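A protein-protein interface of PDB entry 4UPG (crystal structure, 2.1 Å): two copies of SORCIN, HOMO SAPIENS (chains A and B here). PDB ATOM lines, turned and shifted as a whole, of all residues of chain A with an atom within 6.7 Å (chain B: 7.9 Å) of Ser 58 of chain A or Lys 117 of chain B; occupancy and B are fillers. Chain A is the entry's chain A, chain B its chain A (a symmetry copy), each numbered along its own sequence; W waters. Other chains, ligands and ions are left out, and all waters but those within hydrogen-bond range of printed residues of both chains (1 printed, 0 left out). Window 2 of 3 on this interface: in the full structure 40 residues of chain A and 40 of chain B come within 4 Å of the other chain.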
ATOM      1  N   GLN A  19     -23.455 -31.198  -7.997  1.00  0.00           N
ATOM      2  CA  GLN A  19     -24.378 -30.318  -8.693  1.00  0.00           C
ATOM      3  C   GLN A  19     -25.004 -30.990  -9.901  1.00  0.00           C
ATOM      4  O   GLN A  19     -24.507 -31.998 -10.421  1.00  0.00           O
ATOM      5  CB  GLN A  19     -23.682 -29.012  -9.064  1.00  0.00           C
ATOM      6  CG  GLN A  19     -23.239 -28.270  -7.803  1.00  0.00           C
ATOM      7  CD  GLN A  19     -22.927 -26.827  -8.092  1.00  0.00           C
ATOM      8  OE1 GLN A  19     -23.803 -26.064  -8.516  1.00  0.00           O
ATOM      9  NE2 GLN A  19     -21.670 -26.440  -7.884  1.00  0.00           N
ATOM     10  N   ARG A  47     -33.751 -25.420 -17.959  1.00  0.00           N
ATOM     11  CA  ARG A  47     -32.721 -24.386 -18.066  1.00  0.00           C
ATOM     12  C   ARG A  47     -33.113 -23.055 -17.413  1.00  0.00           C
ATOM     13  O   ARG A  47     -32.310 -22.440 -16.716  1.00  0.00           O
ATOM     14  CB  ARG A  47     -32.394 -24.111 -19.503  1.00  0.00           C
ATOM     15  CG  ARG A  47     -31.737 -25.254 -20.233  1.00  0.00           C
ATOM     16  CD  ARG A  47     -31.489 -24.779 -21.662  1.00  0.00           C
ATOM     17  NE  ARG A  47     -31.079 -25.818 -22.581  1.00  0.00           N
ATOM     18  CZ  ARG A  47     -29.857 -26.298 -22.698  1.00  0.00           C
ATOM     19  NH1 ARG A  47     -28.866 -25.864 -21.914  1.00  0.00           N
ATOM     20  NH2 ARG A  47     -29.622 -27.246 -23.599  1.00  0.00           N
ATOM     21  N   VAL A  50     -32.881 -23.612 -13.583  1.00  0.00           N
ATOM     22  CA  VAL A  50     -31.488 -23.530 -13.160  1.00  0.00           C
ATOM     23  C   VAL A  50     -30.992 -22.085 -13.004  1.00  0.00           C
ATOM     24  O   VAL A  50     -30.350 -21.773 -11.999  1.00  0.00           O
ATOM     25  CB  VAL A  50     -30.537 -24.288 -14.098  1.00  0.00           C
ATOM     26  CG1 VAL A  50     -29.087 -24.050 -13.671  1.00  0.00           C
ATOM     27  CG2 VAL A  50     -30.851 -25.785 -14.056  1.00  0.00           C
ATOM     28  N   SER A  51     -31.308 -21.219 -13.965  1.00  0.00           N
ATOM     29  CA  SER A  51     -30.898 -19.812 -13.916  1.00  0.00           C
ATOM     30  C   SER A  51     -31.615 -19.050 -12.805  1.00  0.00           C
ATOM     31  O   SER A  51     -31.023 -18.198 -12.149  1.00  0.00           O
ATOM     32  CB  SER A  51     -31.183 -19.131 -15.252  1.00  0.00           C
ATOM     33  OG  SER A  51     -30.557 -19.832 -16.312  1.00  0.00           O
ATOM     34  N   ASP A  54     -29.741 -20.591  -9.506  1.00  0.00           N
ATOM     35  CA  ASP A  54     -28.303 -20.353  -9.337  1.00  0.00           C
ATOM     36  C   ASP A  54     -27.936 -18.899  -9.394  1.00  0.00           C
ATOM     37  O   ASP A  54     -26.983 -18.505  -8.760  1.00  0.00           O
ATOM     38  CB  ASP A  54     -27.419 -21.220 -10.227  1.00  0.00           C
ATOM     39  CG  ASP A  54     -27.451 -20.874 -11.680  1.00  0.00           C
ATOM     40  OD1 ASP A  54     -27.850 -19.759 -12.123  1.00  0.00           O
ATOM     41  OD2 ASP A  54     -26.984 -21.789 -12.406  1.00  0.00           O
ATOM     42  N   ARG A  55     -28.716 -18.108 -10.130  1.00  0.00           N
ATOM     43  CA  ARG A  55     -28.499 -16.664 -10.260  1.00  0.00           C
ATOM     44  C   ARG A  55     -27.015 -16.288 -10.457  1.00  0.00           C
ATOM     45  O   ARG A  55     -26.571 -15.270  -9.924  1.00  0.00           O
ATOM     46  CB  ARG A  55     -29.062 -15.931  -9.032  1.00  0.00           C
ATOM     47  CG  ARG A  55     -30.524 -16.229  -8.757  1.00  0.00           C
ATOM     48  CD  ARG A  55     -31.052 -15.420  -7.579  1.00  0.00           C
ATOM     49  NE  ARG A  55     -31.104 -13.998  -7.918  1.00  0.00           N
ATOM     50  CZ  ARG A  55     -31.488 -13.029  -7.094  1.00  0.00           C
ATOM     51  NH1 ARG A  55     -31.858 -13.309  -5.848  1.00  0.00           N
ATOM     52  NH2 ARG A  55     -31.494 -11.775  -7.518  1.00  0.00           N
ATOM     53  N   ASP A  56     -26.275 -17.101 -11.219  1.00  0.00           N
ATOM     54  CA  ASP A  56     -24.832 -16.883 -11.440  1.00  0.00           C
ATOM     55  C   ASP A  56     -24.310 -17.434 -12.783  1.00  0.00           C
ATOM     56  O   ASP A  56     -23.095 -17.471 -13.017  1.00  0.00           O
ATOM     57  CB  ASP A  56     -24.000 -17.471 -10.269  1.00  0.00           C
ATOM     58  CG  ASP A  56     -24.080 -19.019 -10.172  1.00  0.00           C
ATOM     59  OD1 ASP A  56     -24.792 -19.669 -10.972  1.00  0.00           O
ATOM     60  OD2 ASP A  56     -23.402 -19.598  -9.292  1.00  0.00           O
ATOM     61  N   MET A  57     -25.219 -17.888 -13.645  1.00  0.00           N
ATOM     62  CA  MET A  57     -24.854 -18.406 -14.975  1.00  0.00           C
ATOM     63  C   MET A  57     -23.780 -19.526 -14.973  1.00  0.00           C
ATOM     64  O   MET A  57     -23.006 -19.644 -15.922  1.00  0.00           O
ATOM     65  CB  MET A  57     -24.414 -17.240 -15.884  1.00  0.00           C
ATOM     66  CG  MET A  57     -25.485 -16.171 -16.143  1.00  0.00           C
ATOM     67  SD  MET A  57     -25.431 -14.581 -15.267  1.00  0.00           S
ATOM     68  CE  MET A  57     -23.707 -14.358 -14.831  1.00  0.00           C
ATOM     69  N   SER A  58     -23.731 -20.352 -13.918  1.00  0.00           N
ATOM     70  CA  SER A  58     -22.898 -21.566 -13.939  1.00  0.00           C
ATOM     71  C   SER A  58     -23.575 -22.684 -14.735  1.00  0.00           C
ATOM     72  O   SER A  58     -22.937 -23.653 -15.130  1.00  0.00           O
ATOM     73  CB  SER A  58     -22.618 -22.060 -12.519  1.00  0.00           C
ATOM     74  OG  SER A  58     -23.827 -22.398 -11.854  1.00  0.00           O
ATOM     75  N   GLY A  59     -24.877 -22.554 -14.946  1.00  0.00           N
ATOM     76  CA  GLY A  59     -25.684 -23.624 -15.534  1.00  0.00           C
ATOM     77  C   GLY A  59     -25.913 -24.841 -14.641  1.00  0.00           C
ATOM     78  O   GLY A  59     -26.333 -25.874 -15.133  1.00  0.00           O
ATOM     79  N   THR A  60     -25.623 -24.735 -13.348  1.00  0.00           N
ATOM     80  CA  THR A  60     -25.793 -25.861 -12.435  1.00  0.00           C
ATOM     81  C   THR A  60     -26.376 -25.373 -11.121  1.00  0.00           C
ATOM     82  O   THR A  60     -26.360 -24.179 -10.810  1.00  0.00           O
ATOM     83  CB  THR A  60     -24.469 -26.601 -12.090  1.00  0.00           C
ATOM     84  OG1 THR A  60     -23.686 -25.760 -11.253  1.00  0.00           O
ATOM     85  CG2 THR A  60     -23.653 -26.999 -13.346  1.00  0.00           C
ATOM     86  N   MET A  61     -26.899 -26.320 -10.356  1.00  0.00           N
ATOM     87  CA  MET A  61     -27.453 -26.039  -9.046  1.00  0.00           C
ATOM     88  C   MET A  61     -27.210 -27.184  -8.060  1.00  0.00           C
ATOM     89  O   MET A  61     -27.047 -28.335  -8.453  1.00  0.00           O
ATOM     90  CB  MET A  61     -28.949 -25.740  -9.185  1.00  0.00           C
ATOM     91  CG  MET A  61     -29.803 -26.826  -9.829  1.00  0.00           C
ATOM     92  SD  MET A  61     -31.547 -26.291 -10.009  1.00  0.00           S
ATOM     93  CE  MET A  61     -32.003 -26.460  -8.328  1.00  0.00           C
ATOM     94  N   PRO B  93     -18.850 -23.762 -27.822  1.00  0.00           N
ATOM     95  CA  PRO B  93     -18.858 -22.407 -27.264  1.00  0.00           C
ATOM     96  C   PRO B  93     -17.820 -21.438 -27.840  1.00  0.00           C
ATOM     97  O   PRO B  93     -18.096 -20.247 -27.938  1.00  0.00           O
ATOM     98  CB  PRO B  93     -18.624 -22.653 -25.780  1.00  0.00           C
ATOM     99  CG  PRO B  93     -19.309 -23.940 -25.537  1.00  0.00           C
ATOM    100  CD  PRO B  93     -19.008 -24.774 -26.758  1.00  0.00           C
ATOM    101  N   LEU B  96     -19.289 -20.485 -31.238  1.00  0.00           N
ATOM    102  CA  LEU B  96     -20.423 -19.594 -30.944  1.00  0.00           C
ATOM    103  C   LEU B  96     -19.984 -18.157 -30.670  1.00  0.00           C
ATOM    104  O   LEU B  96     -20.574 -17.210 -31.205  1.00  0.00           O
ATOM    105  CB  LEU B  96     -21.239 -20.119 -29.743  1.00  0.00           C
ATOM    106  CG  LEU B  96     -22.510 -19.314 -29.393  1.00  0.00           C
ATOM    107  CD1 LEU B  96     -23.513 -19.280 -30.542  1.00  0.00           C
ATOM    108  CD2 LEU B  96     -23.172 -19.894 -28.157  1.00  0.00           C
ATOM    109  N   ALA B 111     -20.896 -11.988 -20.940  1.00  0.00           N
ATOM    110  CA  ALA B 111     -22.151 -12.044 -21.709  1.00  0.00           C
ATOM    111  C   ALA B 111     -22.170 -13.326 -22.553  1.00  0.00           C
ATOM    112  O   ALA B 111     -23.163 -14.043 -22.595  1.00  0.00           O
ATOM    113  CB  ALA B 111     -22.316 -10.808 -22.579  1.00  0.00           C
ATOM    114  N   VAL B 112     -21.044 -13.637 -23.174  1.00  0.00           N
ATOM    115  CA  VAL B 112     -20.928 -14.829 -24.014  1.00  0.00           C
ATOM    116  C   VAL B 112     -21.060 -16.134 -23.212  1.00  0.00           C
ATOM    117  O   VAL B 112     -21.725 -17.083 -23.649  1.00  0.00           O
ATOM    118  CB  VAL B 112     -19.617 -14.800 -24.786  1.00  0.00           C
ATOM    119  CG1 VAL B 112     -19.437 -16.090 -25.563  1.00  0.00           C
ATOM    120  CG2 VAL B 112     -19.611 -13.597 -25.733  1.00  0.00           C
ATOM    121  N   ASN B 113     -20.427 -16.152 -22.042  1.00  0.00           N
ATOM    122  CA  ASN B 113     -20.537 -17.238 -21.091  1.00  0.00           C
ATOM    123  C   ASN B 113     -21.969 -17.426 -20.615  1.00  0.00           C
ATOM    124  O   ASN B 113     -22.454 -18.551 -20.515  1.00  0.00           O
ATOM    125  CB  ASN B 113     -19.657 -16.933 -19.872  1.00  0.00           C
ATOM    126  CG  ASN B 113     -19.501 -18.128 -18.958  1.00  0.00           C
ATOM    127  OD1 ASN B 113     -20.183 -18.243 -17.934  1.00  0.00           O
ATOM    128  ND2 ASN B 113     -18.622 -19.044 -19.345  1.00  0.00           N
ATOM    129  N   SER B 114     -22.638 -16.331 -20.286  1.00  0.00           N
ATOM    130  CA  SER B 114     -24.068 -16.386 -19.968  1.00  0.00           C
ATOM    131  C   SER B 114     -24.815 -17.166 -21.076  1.00  0.00           C
ATOM    132  O   SER B 114     -25.649 -18.052 -20.809  1.00  0.00           O
ATOM    133  CB  SER B 114     -24.644 -14.965 -19.818  1.00  0.00           C
ATOM    134  OG  SER B 114     -26.078 -14.957 -19.689  1.00  0.00           O
ATOM    135  N   ILE B 115     -24.487 -16.839 -22.324  1.00  0.00           N
ATOM    136  CA  ILE B 115     -25.199 -17.384 -23.493  1.00  0.00           C
ATOM    137  C   ILE B 115     -24.827 -18.846 -23.762  1.00  0.00           C
ATOM    138  O   ILE B 115     -25.694 -19.689 -24.085  1.00  0.00           O
ATOM    139  CB  ILE B 115     -24.940 -16.483 -24.714  1.00  0.00           C
ATOM    140  CG1 ILE B 115     -25.622 -15.139 -24.482  1.00  0.00           C
ATOM    141  CG2 ILE B 115     -25.459 -17.132 -25.987  1.00  0.00           C
ATOM    142  CD1 ILE B 115     -25.064 -13.999 -25.296  1.00  0.00           C
ATOM    143  N   ALA B 116     -23.557 -19.181 -23.566  1.00  0.00           N
ATOM    144  CA  ALA B 116     -23.111 -20.566 -23.797  1.00  0.00           C
ATOM    145  C   ALA B 116     -23.786 -21.511 -22.797  1.00  0.00           C
ATOM    146  O   ALA B 116     -24.347 -22.548 -23.171  1.00  0.00           O
ATOM    147  CB  ALA B 116     -21.605 -20.659 -23.684  1.00  0.00           C
ATOM    148  N   LYS B 117     -23.771 -21.136 -21.527  1.00  0.00           N
ATOM    149  CA  LYS B 117     -24.426 -21.940 -20.490  1.00  0.00           C
ATOM    150  C   LYS B 117     -25.902 -22.073 -20.710  1.00  0.00           C
ATOM    151  O   LYS B 117     -26.510 -23.095 -20.383  1.00  0.00           O
ATOM    152  CB  LYS B 117     -24.226 -21.326 -19.105  1.00  0.00           C
ATOM    153  CG  LYS B 117     -23.160 -22.011 -18.291  1.00  0.00           C
ATOM    154  CD  LYS B 117     -21.783 -21.856 -18.891  1.00  0.00           C
ATOM    155  CE  LYS B 117     -20.775 -22.386 -17.889  1.00  0.00           C
ATOM    156  NZ  LYS B 117     -19.392 -22.366 -18.423  1.00  0.00           N
ATOM    157  N   ARG B 118     -26.505 -21.001 -21.201  1.00  0.00           N
ATOM    158  CA  ARG B 118     -27.931 -20.991 -21.429  1.00  0.00           C
ATOM    159  C   ARG B 118     -28.334 -22.009 -22.497  1.00  0.00           C
ATOM    160  O   ARG B 118     -29.420 -22.560 -22.417  1.00  0.00           O
ATOM    161  CB  ARG B 118     -28.355 -19.575 -21.863  1.00  0.00           C
ATOM    162  CG  ARG B 118     -29.763 -19.454 -22.387  1.00  0.00           C
ATOM    163  CD  ARG B 118     -30.799 -19.728 -21.305  1.00  0.00           C
ATOM    164  NE  ARG B 118     -32.153 -19.587 -21.860  1.00  0.00           N
ATOM    165  CZ  ARG B 118     -32.754 -20.494 -22.610  1.00  0.00           C
ATOM    166  NH1 ARG B 118     -32.155 -21.645 -22.901  1.00  0.00           N
ATOM    167  NH2 ARG B 118     -33.973 -20.268 -23.080  1.00  0.00           N
ATOM    168  N   TYR B 119     -27.501 -22.223 -23.525  1.00  0.00           N
ATOM    169  CA  TYR B 119     -27.933 -23.019 -24.704  1.00  0.00           C
ATOM    170  C   TYR B 119     -27.132 -24.308 -24.951  1.00  0.00           C
ATOM    171  O   TYR B 119     -27.450 -25.074 -25.856  1.00  0.00           O
ATOM    172  CB  TYR B 119     -27.915 -22.161 -26.001  1.00  0.00           C
ATOM    173  CG  TYR B 119     -28.922 -21.025 -26.018  1.00  0.00           C
ATOM    174  CD1 TYR B 119     -30.278 -21.279 -26.166  1.00  0.00           C
ATOM    175  CD2 TYR B 119     -28.514 -19.698 -25.869  1.00  0.00           C
ATOM    176  CE1 TYR B 119     -31.206 -20.239 -26.180  1.00  0.00           C
ATOM    177  CE2 TYR B 119     -29.428 -18.665 -25.877  1.00  0.00           C
ATOM    178  CZ  TYR B 119     -30.771 -18.940 -26.037  1.00  0.00           C
ATOM    179  OH  TYR B 119     -31.681 -17.923 -25.996  1.00  0.00           O
ATOM    180  N   SER B 120     -26.090 -24.570 -24.185  1.00  0.00           N
ATOM    181  CA  SER B 120     -25.269 -25.731 -24.514  1.00  0.00           C
ATOM    182  C   SER B 120     -25.743 -26.989 -23.773  1.00  0.00           C
ATOM    183  O   SER B 120     -26.204 -26.913 -22.644  1.00  0.00           O
ATOM    184  CB  SER B 120     -23.799 -25.436 -24.240  1.00  0.00           C
ATOM    185  OG  SER B 120     -23.569 -25.509 -22.862  1.00  0.00           O
ATOM    186  N   THR B 121     -25.672 -28.135 -24.443  1.00  0.00           N
ATOM    187  CA  THR B 121     -25.797 -29.446 -23.781  1.00  0.00           C
ATOM    188  C   THR B 121     -24.586 -30.261 -24.223  1.00  0.00           C
ATOM    189  O   THR B 121     -24.332 -30.404 -25.423  1.00  0.00           O
ATOM    190  CB  THR B 121     -27.086 -30.227 -24.167  1.00  0.00           C
ATOM    191  OG1 THR B 121     -28.257 -29.511 -23.758  1.00  0.00           O
ATOM    192  CG2 THR B 121     -27.119 -31.582 -23.469  1.00  0.00           C
ATOM    193  N   ILE B 125     -23.936 -26.523 -28.956  1.00  0.00           N
ATOM    194  CA  ILE B 125     -25.102 -25.680 -29.224  1.00  0.00           C
ATOM    195  C   ILE B 125     -25.688 -26.079 -30.594  1.00  0.00           C
ATOM    196  O   ILE B 125     -25.026 -25.975 -31.612  1.00  0.00           O
ATOM    197  CB  ILE B 125     -24.728 -24.171 -29.200  1.00  0.00           C
ATOM    198  CG1 ILE B 125     -24.240 -23.758 -27.801  1.00  0.00           C
ATOM    199  CG2 ILE B 125     -25.916 -23.300 -29.609  1.00  0.00           C
ATOM    200  CD1 ILE B 125     -22.738 -23.799 -27.580  1.00  0.00           C
HETATM  201  O   HOH W   1     -28.505 -24.318 -19.068  1.00  0.00           O
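The backbone carbonyl oxygen (O) of Ser 120 of chain B lies within hydrogen-bond range of the guanidinium group (NH1) of Arg 47 of chain A (3.0 Å).
The side-chain hydroxyl (OG1) of Thr 121 of chain B lies within hydrogen-bond range of the guanidinium group (NH2) of Arg 47 of chain A, at 2.6 Å.
The guanidinium group (NH1) of Arg 47 of chain A sits close to the backbone carbonyl oxygen (O) of Arg 118 of chain B.
O of Ala 116 of chain B is in hydrogen-bond range of OG of Ser 120 of chain B (3.1 Å).
OD2 of Asp 54 of chain A sits at hydrogen-bond distance from OG of Ser 58 of chain A (3.3 Å).
The side-chain hydroxyl (OG) of Ser 58 of chain A is in hydrogen-bond range of the backbone carbonyl oxygen (O) of Thr 60 of chain A (3.3 Å).
The side-chain carboxylate (OD2) of Asp 54 of chain A is in hydrogen-bond range of the backbone NH (N) of Gly 59 of chain A, at 3.4 Å.
The side-chain hydroxyl (OG) of Ser 58 of chain A lies within hydrogen-bond range of the side-chain carboxylate (OD1) of Asp 56 of chain A, 3.0 Å away.
The backbone carbonyl oxygen (O) of Arg 47 of chain A lies within hydrogen-bond range of the side-chain hydroxyl (OG) of Ser 51 of chain A, 3.2 Å away.
Among the printed residues, merely in contact across the chains: Arg 47 of chain A with Lys 117 of chain B (3.9 Å), Arg 47 of chain A with Tyr 119 of chain B (3.8 Å), Met 57 of chain A with Asn 113 of chain B (3.7 Å), Met 57 of chain A with Ser 114 of chain B (3.8 Å), Met 57 of chain A with Lys 117 of chain B (3.4 Å), Ser 58 of chain A with Lys 117 of chain B (3.6 Å) and Gly 59 of chain A with Lys 117 of chain B (3.8 Å).
Ser 58 of chain A touches just one residue of chain B: Lys 117.
Printed residues of chain A within 4 Å of Lys 117 of chain B: Arg 47, Met 57, Ser 58 and Gly 59.
Of the printed residues of chain B, Arg 47 of chain A touches Lys 117 (3.9 Å), Arg 118 (3.1 Å), Tyr 119 (3.8 Å), Ser 120 (3.0 Å) and Thr 121 (2.6 Å).
Of the printed residues of chain B, Gly 59 of chain A touches Lys 117.
Of the printed residues of chain A, Ser 114 of chain B touches Met 57 (3.8 Å).
Pro 93 of chain B touches none of the printed residues of chain A.
Met 61 of chain A touches none of the printed residues of chain B.
Of the 14 printed residues of chain B, 7 touch a printed residue of chain A.
Of the 12 printed residues of chain A, 4 touch a printed residue of chain B.
Hydrophobic or aromatic side chains of chain A within 4 Å of the printed part of chain B: Met 57.
Among the printed residues, no Asp or Glu carboxylate lies within 4 Å of a Lys or Arg side-chain nitrogen of the other chain.
No position is printed for both chains.
Water W1 bridges O of Lys 117 of chain B (2.7 Å) and NH1 of Arg 47 of chain A (3.3 Å).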
